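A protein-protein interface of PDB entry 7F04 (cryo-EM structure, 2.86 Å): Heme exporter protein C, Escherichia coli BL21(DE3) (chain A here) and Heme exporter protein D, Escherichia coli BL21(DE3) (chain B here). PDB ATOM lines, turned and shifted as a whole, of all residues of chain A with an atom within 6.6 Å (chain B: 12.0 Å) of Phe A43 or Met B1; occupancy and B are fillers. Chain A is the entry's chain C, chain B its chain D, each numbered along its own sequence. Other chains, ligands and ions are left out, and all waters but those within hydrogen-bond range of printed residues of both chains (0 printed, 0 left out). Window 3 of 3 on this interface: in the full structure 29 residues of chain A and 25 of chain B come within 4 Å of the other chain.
Phe A43 touches just these residues of chain B: Met B1 (3.5 Å), Thr B2 (3.2 Å), Pro B3 (3.8 Å) and Ala B4 (3.3 Å). Of chain A, only Phe A43 (3.5 Å) comes within 4 Å of Met B1. Gly A42 touches just these residues of chain B: Pro B3, Ala B4, Phe B5 and Phe B12. Of chain B, only Ala B4 (3.4 Å) comes within 4 Å of Ala A44. Of the printed residues of chain A, Thr B2 touches Phe A43. Of the printed residues of chain A, Val B21 touches Phe A41. Of the printed residues of chain A, Ala B4 touches Gly A42, Phe A43, Ala A44 and Arg A55. Phe B11 touches none of the printed residues of chain A. Ala B13 touches none of the printed residues of chain A. The nearest printed residue of chain A that does not touch Met B1 is Trp A39 (8.6 Å).
O of Gly A42 lies within hydrogen-bond range of N of Ala B4 (2.9 Å).
The backbone carbonyl oxygen (O) of Trp A39 sits at hydrogen-bond distance from the backbone NH (N) of Ala A44. NH2 of Arg A55 sits at hydrogen-bond distance from O of Ala A44 (3.0 Å).
Of the 13 printed residues of chain B, 7 touch a printed residue of chain A. Hydrophobic or aromatic side chains of chain B within 4 Å of the printed part of chain A: Ala B4, Phe B5, Phe B12 and Val B21. Of the 10 printed residues of chain A, 5 touch a printed residue of chain B. Among the printed residues, no Asp or Glu carboxylate lies within 4 Å of a Lys or Arg side-chain nitrogen of the other chain.
Among the printed residues, pairs that only touch across the chains: Phe A41 with Phe B12 (3.6 Å), Phe A41 with Val B21 (3.8 Å), Gly A42 with Pro B3 (3.9 Å), Gly A42 with Phe B5 (3.97 Å), Gly A42 with Phe B12 (3.8 Å), Phe A43 with Met B1 (3.5 Å), Phe A43 with Thr B2 (3.2 Å), Phe A43 with Pro B3 (3.8 Å), Phe A43 with Ala B4 (3.3 Å), Ala A44 with Ala B4 (3.4 Å), Arg A55 with Ala B4 (3.3 Å) and Arg A55 with Phe B5 (3.9 Å).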
ATOM      1  N   TRP A  37      18.527 -26.205  26.763  1.00  0.00           N
ATOM      2  CA  TRP A  37      17.278 -26.948  26.746  1.00  0.00           C
ATOM      3  C   TRP A  37      16.054 -26.058  26.606  1.00  0.00           C
ATOM      4  O   TRP A  37      14.948 -26.577  26.439  1.00  0.00           O
ATOM      5  CB  TRP A  37      17.153 -27.786  28.020  1.00  0.00           C
ATOM      6  CG  TRP A  37      17.925 -29.059  27.972  1.00  0.00           C
ATOM      7  CD1 TRP A  37      18.558 -29.589  26.892  1.00  0.00           C
ATOM      8  CD2 TRP A  37      18.148 -29.967  29.054  1.00  0.00           C
ATOM      9  NE1 TRP A  37      19.163 -30.772  27.231  1.00  0.00           N
ATOM     10  CE2 TRP A  37      18.925 -31.027  28.555  1.00  0.00           C
ATOM     11  CE3 TRP A  37      17.766 -29.987  30.398  1.00  0.00           C
ATOM     12  CZ2 TRP A  37      19.327 -32.094  29.350  1.00  0.00           C
ATOM     13  CZ3 TRP A  37      18.166 -31.048  31.185  1.00  0.00           C
ATOM     14  CH2 TRP A  37      18.939 -32.087  30.659  1.00  0.00           C
ATOM     15  N   ILE A  38      16.212 -24.743  26.703  1.00  0.00           N
ATOM     16  CA  ILE A  38      15.144 -23.831  26.310  1.00  0.00           C
ATOM     17  C   ILE A  38      15.312 -23.396  24.859  1.00  0.00           C
ATOM     18  O   ILE A  38      14.326 -23.243  24.135  1.00  0.00           O
ATOM     19  CB  ILE A  38      15.099 -22.624  27.267  1.00  0.00           C
ATOM     20  CG1 ILE A  38      14.718 -23.078  28.674  1.00  0.00           C
ATOM     21  CG2 ILE A  38      14.104 -21.588  26.781  1.00  0.00           C
ATOM     22  CD1 ILE A  38      14.659 -21.953  29.678  1.00  0.00           C
ATOM     23  N   TRP A  39      16.557 -23.199  24.416  1.00  0.00           N
ATOM     24  CA  TRP A  39      16.819 -22.969  23.000  1.00  0.00           C
ATOM     25  C   TRP A  39      16.364 -24.161  22.172  1.00  0.00           C
ATOM     26  O   TRP A  39      15.609 -24.012  21.207  1.00  0.00           O
ATOM     27  CB  TRP A  39      18.309 -22.704  22.788  1.00  0.00           C
ATOM     28  CG  TRP A  39      18.638 -22.002  21.508  1.00  0.00           C
ATOM     29  CD1 TRP A  39      17.856 -21.909  20.400  1.00  0.00           C
ATOM     30  CD2 TRP A  39      19.846 -21.298  21.208  1.00  0.00           C
ATOM     31  NE1 TRP A  39      18.497 -21.188  19.428  1.00  0.00           N
ATOM     32  CE2 TRP A  39      19.723 -20.800  19.900  1.00  0.00           C
ATOM     33  CE3 TRP A  39      21.018 -21.038  21.921  1.00  0.00           C
ATOM     34  CZ2 TRP A  39      20.727 -20.059  19.286  1.00  0.00           C
ATOM     35  CZ3 TRP A  39      22.015 -20.301  21.312  1.00  0.00           C
ATOM     36  CH2 TRP A  39      21.863 -19.820  20.008  1.00  0.00           C
ATOM     37  N   GLY A  40      16.819 -25.354  22.533  1.00  0.00           N
ATOM     38  CA  GLY A  40      16.183 -26.559  22.064  1.00  0.00           C
ATOM     39  C   GLY A  40      14.946 -26.817  22.888  1.00  0.00           C
ATOM     40  O   GLY A  40      14.641 -26.094  23.834  1.00  0.00           O
ATOM     41  N   PHE A  41      14.214 -27.864  22.517  1.00  0.00           N
ATOM     42  CA  PHE A  41      13.039 -28.282  23.279  1.00  0.00           C
ATOM     43  C   PHE A  41      12.053 -27.129  23.451  1.00  0.00           C
ATOM     44  O   PHE A  41      11.604 -26.827  24.558  1.00  0.00           O
ATOM     45  CB  PHE A  41      13.447 -28.842  24.644  1.00  0.00           C
ATOM     46  CG  PHE A  41      13.672 -30.319  24.656  1.00  0.00           C
ATOM     47  CD1 PHE A  41      12.623 -31.194  24.447  1.00  0.00           C
ATOM     48  CD2 PHE A  41      14.931 -30.836  24.894  1.00  0.00           C
ATOM     49  CE1 PHE A  41      12.828 -32.556  24.465  1.00  0.00           C
ATOM     50  CE2 PHE A  41      15.143 -32.195  24.912  1.00  0.00           C
ATOM     51  CZ  PHE A  41      14.091 -33.058  24.698  1.00  0.00           C
ATOM     52  N   GLY A  42      11.725 -26.464  22.349  1.00  0.00           N
ATOM     53  CA  GLY A  42      10.725 -25.418  22.424  1.00  0.00           C
ATOM     54  C   GLY A  42      10.929 -24.214  21.530  1.00  0.00           C
ATOM     55  O   GLY A  42       9.957 -23.538  21.184  1.00  0.00           O
ATOM     56  N   PHE A  43      12.168 -23.924  21.150  1.00  0.00           N
ATOM     57  CA  PHE A  43      12.455 -22.808  20.255  1.00  0.00           C
ATOM     58  C   PHE A  43      12.982 -23.241  18.899  1.00  0.00           C
ATOM     59  O   PHE A  43      12.563 -22.691  17.879  1.00  0.00           O
ATOM     60  CB  PHE A  43      13.461 -21.851  20.904  1.00  0.00           C
ATOM     61  CG  PHE A  43      12.825 -20.711  21.646  1.00  0.00           C
ATOM     62  CD1 PHE A  43      12.420 -20.863  22.959  1.00  0.00           C
ATOM     63  CD2 PHE A  43      12.637 -19.489  21.031  1.00  0.00           C
ATOM     64  CE1 PHE A  43      11.838 -19.820  23.640  1.00  0.00           C
ATOM     65  CE2 PHE A  43      12.054 -18.443  21.708  1.00  0.00           C
ATOM     66  CZ  PHE A  43      11.654 -18.608  23.014  1.00  0.00           C
ATOM     67  N   ALA A  44      13.888 -24.211  18.860  1.00  0.00           N
ATOM     68  CA  ALA A  44      14.450 -24.656  17.595  1.00  0.00           C
ATOM     69  C   ALA A  44      13.392 -25.389  16.775  1.00  0.00           C
ATOM     70  O   ALA A  44      12.516 -26.048  17.339  1.00  0.00           O
ATOM     71  CB  ALA A  44      15.650 -25.569  17.833  1.00  0.00           C
ATOM     72  N   PRO A  45      13.441 -25.291  15.449  1.00  0.00           N
ATOM     73  CA  PRO A  45      12.478 -26.018  14.615  1.00  0.00           C
ATOM     74  C   PRO A  45      12.736 -27.516  14.646  1.00  0.00           C
ATOM     75  O   PRO A  45      13.750 -27.999  15.153  1.00  0.00           O
ATOM     76  CB  PRO A  45      12.707 -25.443  13.214  1.00  0.00           C
ATOM     77  CG  PRO A  45      13.413 -24.140  13.442  1.00  0.00           C
ATOM     78  CD  PRO A  45      14.256 -24.358  14.657  1.00  0.00           C
ATOM     79  N   ARG A  55      13.641 -33.751  18.720  1.00  0.00           N
ATOM     80  CA  ARG A  55      14.113 -32.896  19.802  1.00  0.00           C
ATOM     81  C   ARG A  55      14.908 -33.653  20.850  1.00  0.00           C
ATOM     82  O   ARG A  55      15.368 -33.036  21.814  1.00  0.00           O
ATOM     83  CB  ARG A  55      12.931 -32.185  20.458  1.00  0.00           C
ATOM     84  CG  ARG A  55      12.073 -31.424  19.473  1.00  0.00           C
ATOM     85  CD  ARG A  55      11.551 -30.136  20.058  1.00  0.00           C
ATOM     86  NE  ARG A  55      10.695 -29.436  19.112  1.00  0.00           N
ATOM     87  CZ  ARG A  55      10.939 -28.222  18.641  1.00  0.00           C
ATOM     88  NH1 ARG A  55      12.002 -27.536  19.020  1.00  0.00           N
ATOM     89  NH2 ARG A  55      10.095 -27.683  17.767  1.00  0.00           N
ATOM     90  N   MET B   1      12.656 -15.084  21.076  1.00  0.00           N
ATOM     91  CA  MET B   1      11.512 -14.228  20.798  1.00  0.00           C
ATOM     92  C   MET B   1      10.496 -14.960  19.932  1.00  0.00           C
ATOM     93  O   MET B   1       9.299 -14.687  19.997  1.00  0.00           O
ATOM     94  CB  MET B   1      11.961 -12.934  20.114  1.00  0.00           C
ATOM     95  CG  MET B   1      10.830 -11.981  19.758  1.00  0.00           C
ATOM     96  SD  MET B   1      11.418 -10.366  19.213  1.00  0.00           S
ATOM     97  CE  MET B   1      12.069  -9.706  20.746  1.00  0.00           C
ATOM     98  N   THR B   2      10.978 -15.901  19.127  1.00  0.00           N
ATOM     99  CA  THR B   2      10.127 -16.662  18.211  1.00  0.00           C
ATOM    100  C   THR B   2      10.116 -18.123  18.628  1.00  0.00           C
ATOM    101  O   THR B   2      11.061 -18.868  18.315  1.00  0.00           O
ATOM    102  CB  THR B   2      10.617 -16.522  16.772  1.00  0.00           C
ATOM    103  OG1 THR B   2      11.990 -16.919  16.693  1.00  0.00           O
ATOM    104  CG2 THR B   2      10.485 -15.080  16.305  1.00  0.00           C
ATOM    105  N   PRO B   3       9.082 -18.584  19.328  1.00  0.00           N
ATOM    106  CA  PRO B   3       9.046 -19.985  19.753  1.00  0.00           C
ATOM    107  C   PRO B   3       8.725 -20.906  18.589  1.00  0.00           C
ATOM    108  O   PRO B   3       8.315 -20.475  17.508  1.00  0.00           O
ATOM    109  CB  PRO B   3       7.934 -20.016  20.810  1.00  0.00           C
ATOM    110  CG  PRO B   3       7.554 -18.575  21.056  1.00  0.00           C
ATOM    111  CD  PRO B   3       7.916 -17.833  19.816  1.00  0.00           C
ATOM    112  N   ALA B   4       8.924 -22.199  18.825  1.00  0.00           N
ATOM    113  CA  ALA B   4       8.657 -23.226  17.827  1.00  0.00           C
ATOM    114  C   ALA B   4       7.248 -23.792  17.918  1.00  0.00           C
ATOM    115  O   ALA B   4       6.919 -24.716  17.169  1.00  0.00           O
ATOM    116  CB  ALA B   4       9.673 -24.366  17.951  1.00  0.00           C
ATOM    117  N   PHE B   5       6.414 -23.271  18.809  1.00  0.00           N
ATOM    118  CA  PHE B   5       5.047 -23.741  18.965  1.00  0.00           C
ATOM    119  C   PHE B   5       4.095 -22.554  18.942  1.00  0.00           C
ATOM    120  O   PHE B   5       4.429 -21.466  19.420  1.00  0.00           O
ATOM    121  CB  PHE B   5       4.883 -24.537  20.262  1.00  0.00           C
ATOM    122  CG  PHE B   5       5.573 -25.870  20.241  1.00  0.00           C
ATOM    123  CD1 PHE B   5       4.916 -26.998  19.792  1.00  0.00           C
ATOM    124  CD2 PHE B   5       6.886 -25.989  20.652  1.00  0.00           C
ATOM    125  CE1 PHE B   5       5.553 -28.220  19.770  1.00  0.00           C
ATOM    126  CE2 PHE B   5       7.526 -27.210  20.630  1.00  0.00           C
ATOM    127  CZ  PHE B   5       6.858 -28.325  20.189  1.00  0.00           C
ATOM    128  N   ALA B   6       2.906 -22.774  18.373  1.00  0.00           N
ATOM    129  CA  ALA B   6       1.940 -21.692  18.234  1.00  0.00           C
ATOM    130  C   ALA B   6       1.391 -21.245  19.582  1.00  0.00           C
ATOM    131  O   ALA B   6       1.087 -20.060  19.761  1.00  0.00           O
ATOM    132  CB  ALA B   6       0.798 -22.123  17.314  1.00  0.00           C
ATOM    133  N   SER B   7       1.251 -22.163  20.531  1.00  0.00           N
ATOM    134  CA  SER B   7       0.716 -21.825  21.840  1.00  0.00           C
ATOM    135  C   SER B   7       1.325 -22.763  22.872  1.00  0.00           C
ATOM    136  O   SER B   7       2.309 -23.460  22.604  1.00  0.00           O
ATOM    137  CB  SER B   7      -0.815 -21.884  21.832  1.00  0.00           C
ATOM    138  OG  SER B   7      -1.358 -20.843  21.040  1.00  0.00           O
ATOM    139  N   TRP B   8       0.719 -22.792  24.057  1.00  0.00           N
ATOM    140  CA  TRP B   8       1.263 -23.508  25.202  1.00  0.00           C
ATOM    141  C   TRP B   8       1.013 -25.001  25.106  1.00  0.00           C
ATOM    142  O   TRP B   8       0.669 -25.508  24.035  1.00  0.00           O
ATOM    143  CB  TRP B   8       0.688 -22.954  26.505  1.00  0.00           C
ATOM    144  CG  TRP B   8       1.626 -22.019  27.195  1.00  0.00           C
ATOM    145  CD1 TRP B   8       1.490 -20.672  27.332  1.00  0.00           C
ATOM    146  CD2 TRP B   8       2.849 -22.370  27.849  1.00  0.00           C
ATOM    147  NE1 TRP B   8       2.556 -20.160  28.030  1.00  0.00           N
ATOM    148  CE2 TRP B   8       3.403 -21.185  28.359  1.00  0.00           C
ATOM    149  CE3 TRP B   8       3.527 -23.574  28.053  1.00  0.00           C
ATOM    150  CZ2 TRP B   8       4.606 -21.167  29.061  1.00  0.00           C
ATOM    151  CZ3 TRP B   8       4.717 -23.556  28.747  1.00  0.00           C
ATOM    152  CH2 TRP B   8       5.246 -22.363  29.244  1.00  0.00           C
ATOM    153  N   PHE B  11      -0.397 -27.001  22.526  1.00  0.00           N
ATOM    154  CA  PHE B  11       0.410 -27.281  21.343  1.00  0.00           C
ATOM    155  C   PHE B  11       1.786 -27.811  21.713  1.00  0.00           C
ATOM    156  O   PHE B  11       2.240 -28.812  21.155  1.00  0.00           O
ATOM    157  CB  PHE B  11       0.568 -26.017  20.487  1.00  0.00           C
ATOM    158  CG  PHE B  11      -0.652 -25.655  19.694  1.00  0.00           C
ATOM    159  CD1 PHE B  11      -1.839 -25.327  20.327  1.00  0.00           C
ATOM    160  CD2 PHE B  11      -0.607 -25.624  18.311  1.00  0.00           C
ATOM    161  CE1 PHE B  11      -2.960 -24.986  19.595  1.00  0.00           C
ATOM    162  CE2 PHE B  11      -1.722 -25.284  17.574  1.00  0.00           C
ATOM    163  CZ  PHE B  11      -2.901 -24.964  18.216  1.00  0.00           C
ATOM    164  N   PHE B  12       2.464 -27.147  22.647  1.00  0.00           N
ATOM    165  CA  PHE B  12       3.676 -27.668  23.254  1.00  0.00           C
ATOM    166  C   PHE B  12       3.353 -28.971  23.984  1.00  0.00           C
ATOM    167  O   PHE B  12       2.198 -29.383  24.090  1.00  0.00           O
ATOM    168  CB  PHE B  12       4.264 -26.626  24.211  1.00  0.00           C
ATOM    169  CG  PHE B  12       5.643 -26.953  24.723  1.00  0.00           C
ATOM    170  CD1 PHE B  12       6.744 -26.867  23.895  1.00  0.00           C
ATOM    171  CD2 PHE B  12       5.838 -27.317  26.043  1.00  0.00           C
ATOM    172  CE1 PHE B  12       8.008 -27.157  24.369  1.00  0.00           C
ATOM    173  CE2 PHE B  12       7.100 -27.609  26.519  1.00  0.00           C
ATOM    174  CZ  PHE B  12       8.185 -27.529  25.681  1.00  0.00           C
ATOM    175  N   ALA B  13       4.399 -29.651  24.448  1.00  0.00           N
ATOM    176  CA  ALA B  13       4.245 -30.838  25.284  1.00  0.00           C
ATOM    177  C   ALA B  13       3.554 -31.976  24.541  1.00  0.00           C
ATOM    178  O   ALA B  13       3.302 -33.036  25.120  1.00  0.00           O
ATOM    179  CB  ALA B  13       3.481 -30.504  26.568  1.00  0.00           C
ATOM    180  N   VAL B  21       8.870 -38.345  23.663  1.00  0.00           N
ATOM    181  CA  VAL B  21       9.707 -37.195  23.984  1.00  0.00           C
ATOM    182  C   VAL B  21       9.833 -37.034  25.492  1.00  0.00           C
ATOM    183  O   VAL B  21      10.937 -36.882  26.027  1.00  0.00           O
ATOM    184  CB  VAL B  21       9.142 -35.924  23.328  1.00  0.00           C
ATOM    185  CG1 VAL B  21       9.687 -34.688  24.018  1.00  0.00           C
ATOM    186  CG2 VAL B  21       9.478 -35.902  21.848  1.00  0.00           C
ATOM    187  N   TRP B  22       8.707 -37.076  26.200  1.00  0.00           N
ATOM    188  CA  TRP B  22       8.715 -36.834  27.636  1.00  0.00           C
ATOM    189  C   TRP B  22       9.215 -38.025  28.435  1.00  0.00           C
ATOM    190  O   TRP B  22       9.689 -37.839  29.559  1.00  0.00           O
ATOM    191  CB  TRP B  22       7.319 -36.431  28.105  1.00  0.00           C
ATOM    192  CG  TRP B  22       6.895 -35.097  27.573  1.00  0.00           C
ATOM    193  CD1 TRP B  22       5.791 -34.829  26.824  1.00  0.00           C
ATOM    194  CD2 TRP B  22       7.579 -33.849  27.739  1.00  0.00           C
ATOM    195  NE1 TRP B  22       5.739 -33.494  26.517  1.00  0.00           N
ATOM    196  CE2 TRP B  22       6.826 -32.870  27.068  1.00  0.00           C
ATOM    197  CE3 TRP B  22       8.750 -33.465  28.396  1.00  0.00           C
ATOM    198  CZ2 TRP B  22       7.206 -31.532  27.032  1.00  0.00           C
ATOM    199  CZ3 TRP B  22       9.126 -32.138  28.358  1.00  0.00           C
ATOM    200  CH2 TRP B  22       8.356 -31.188  27.683  1.00  0.00           C
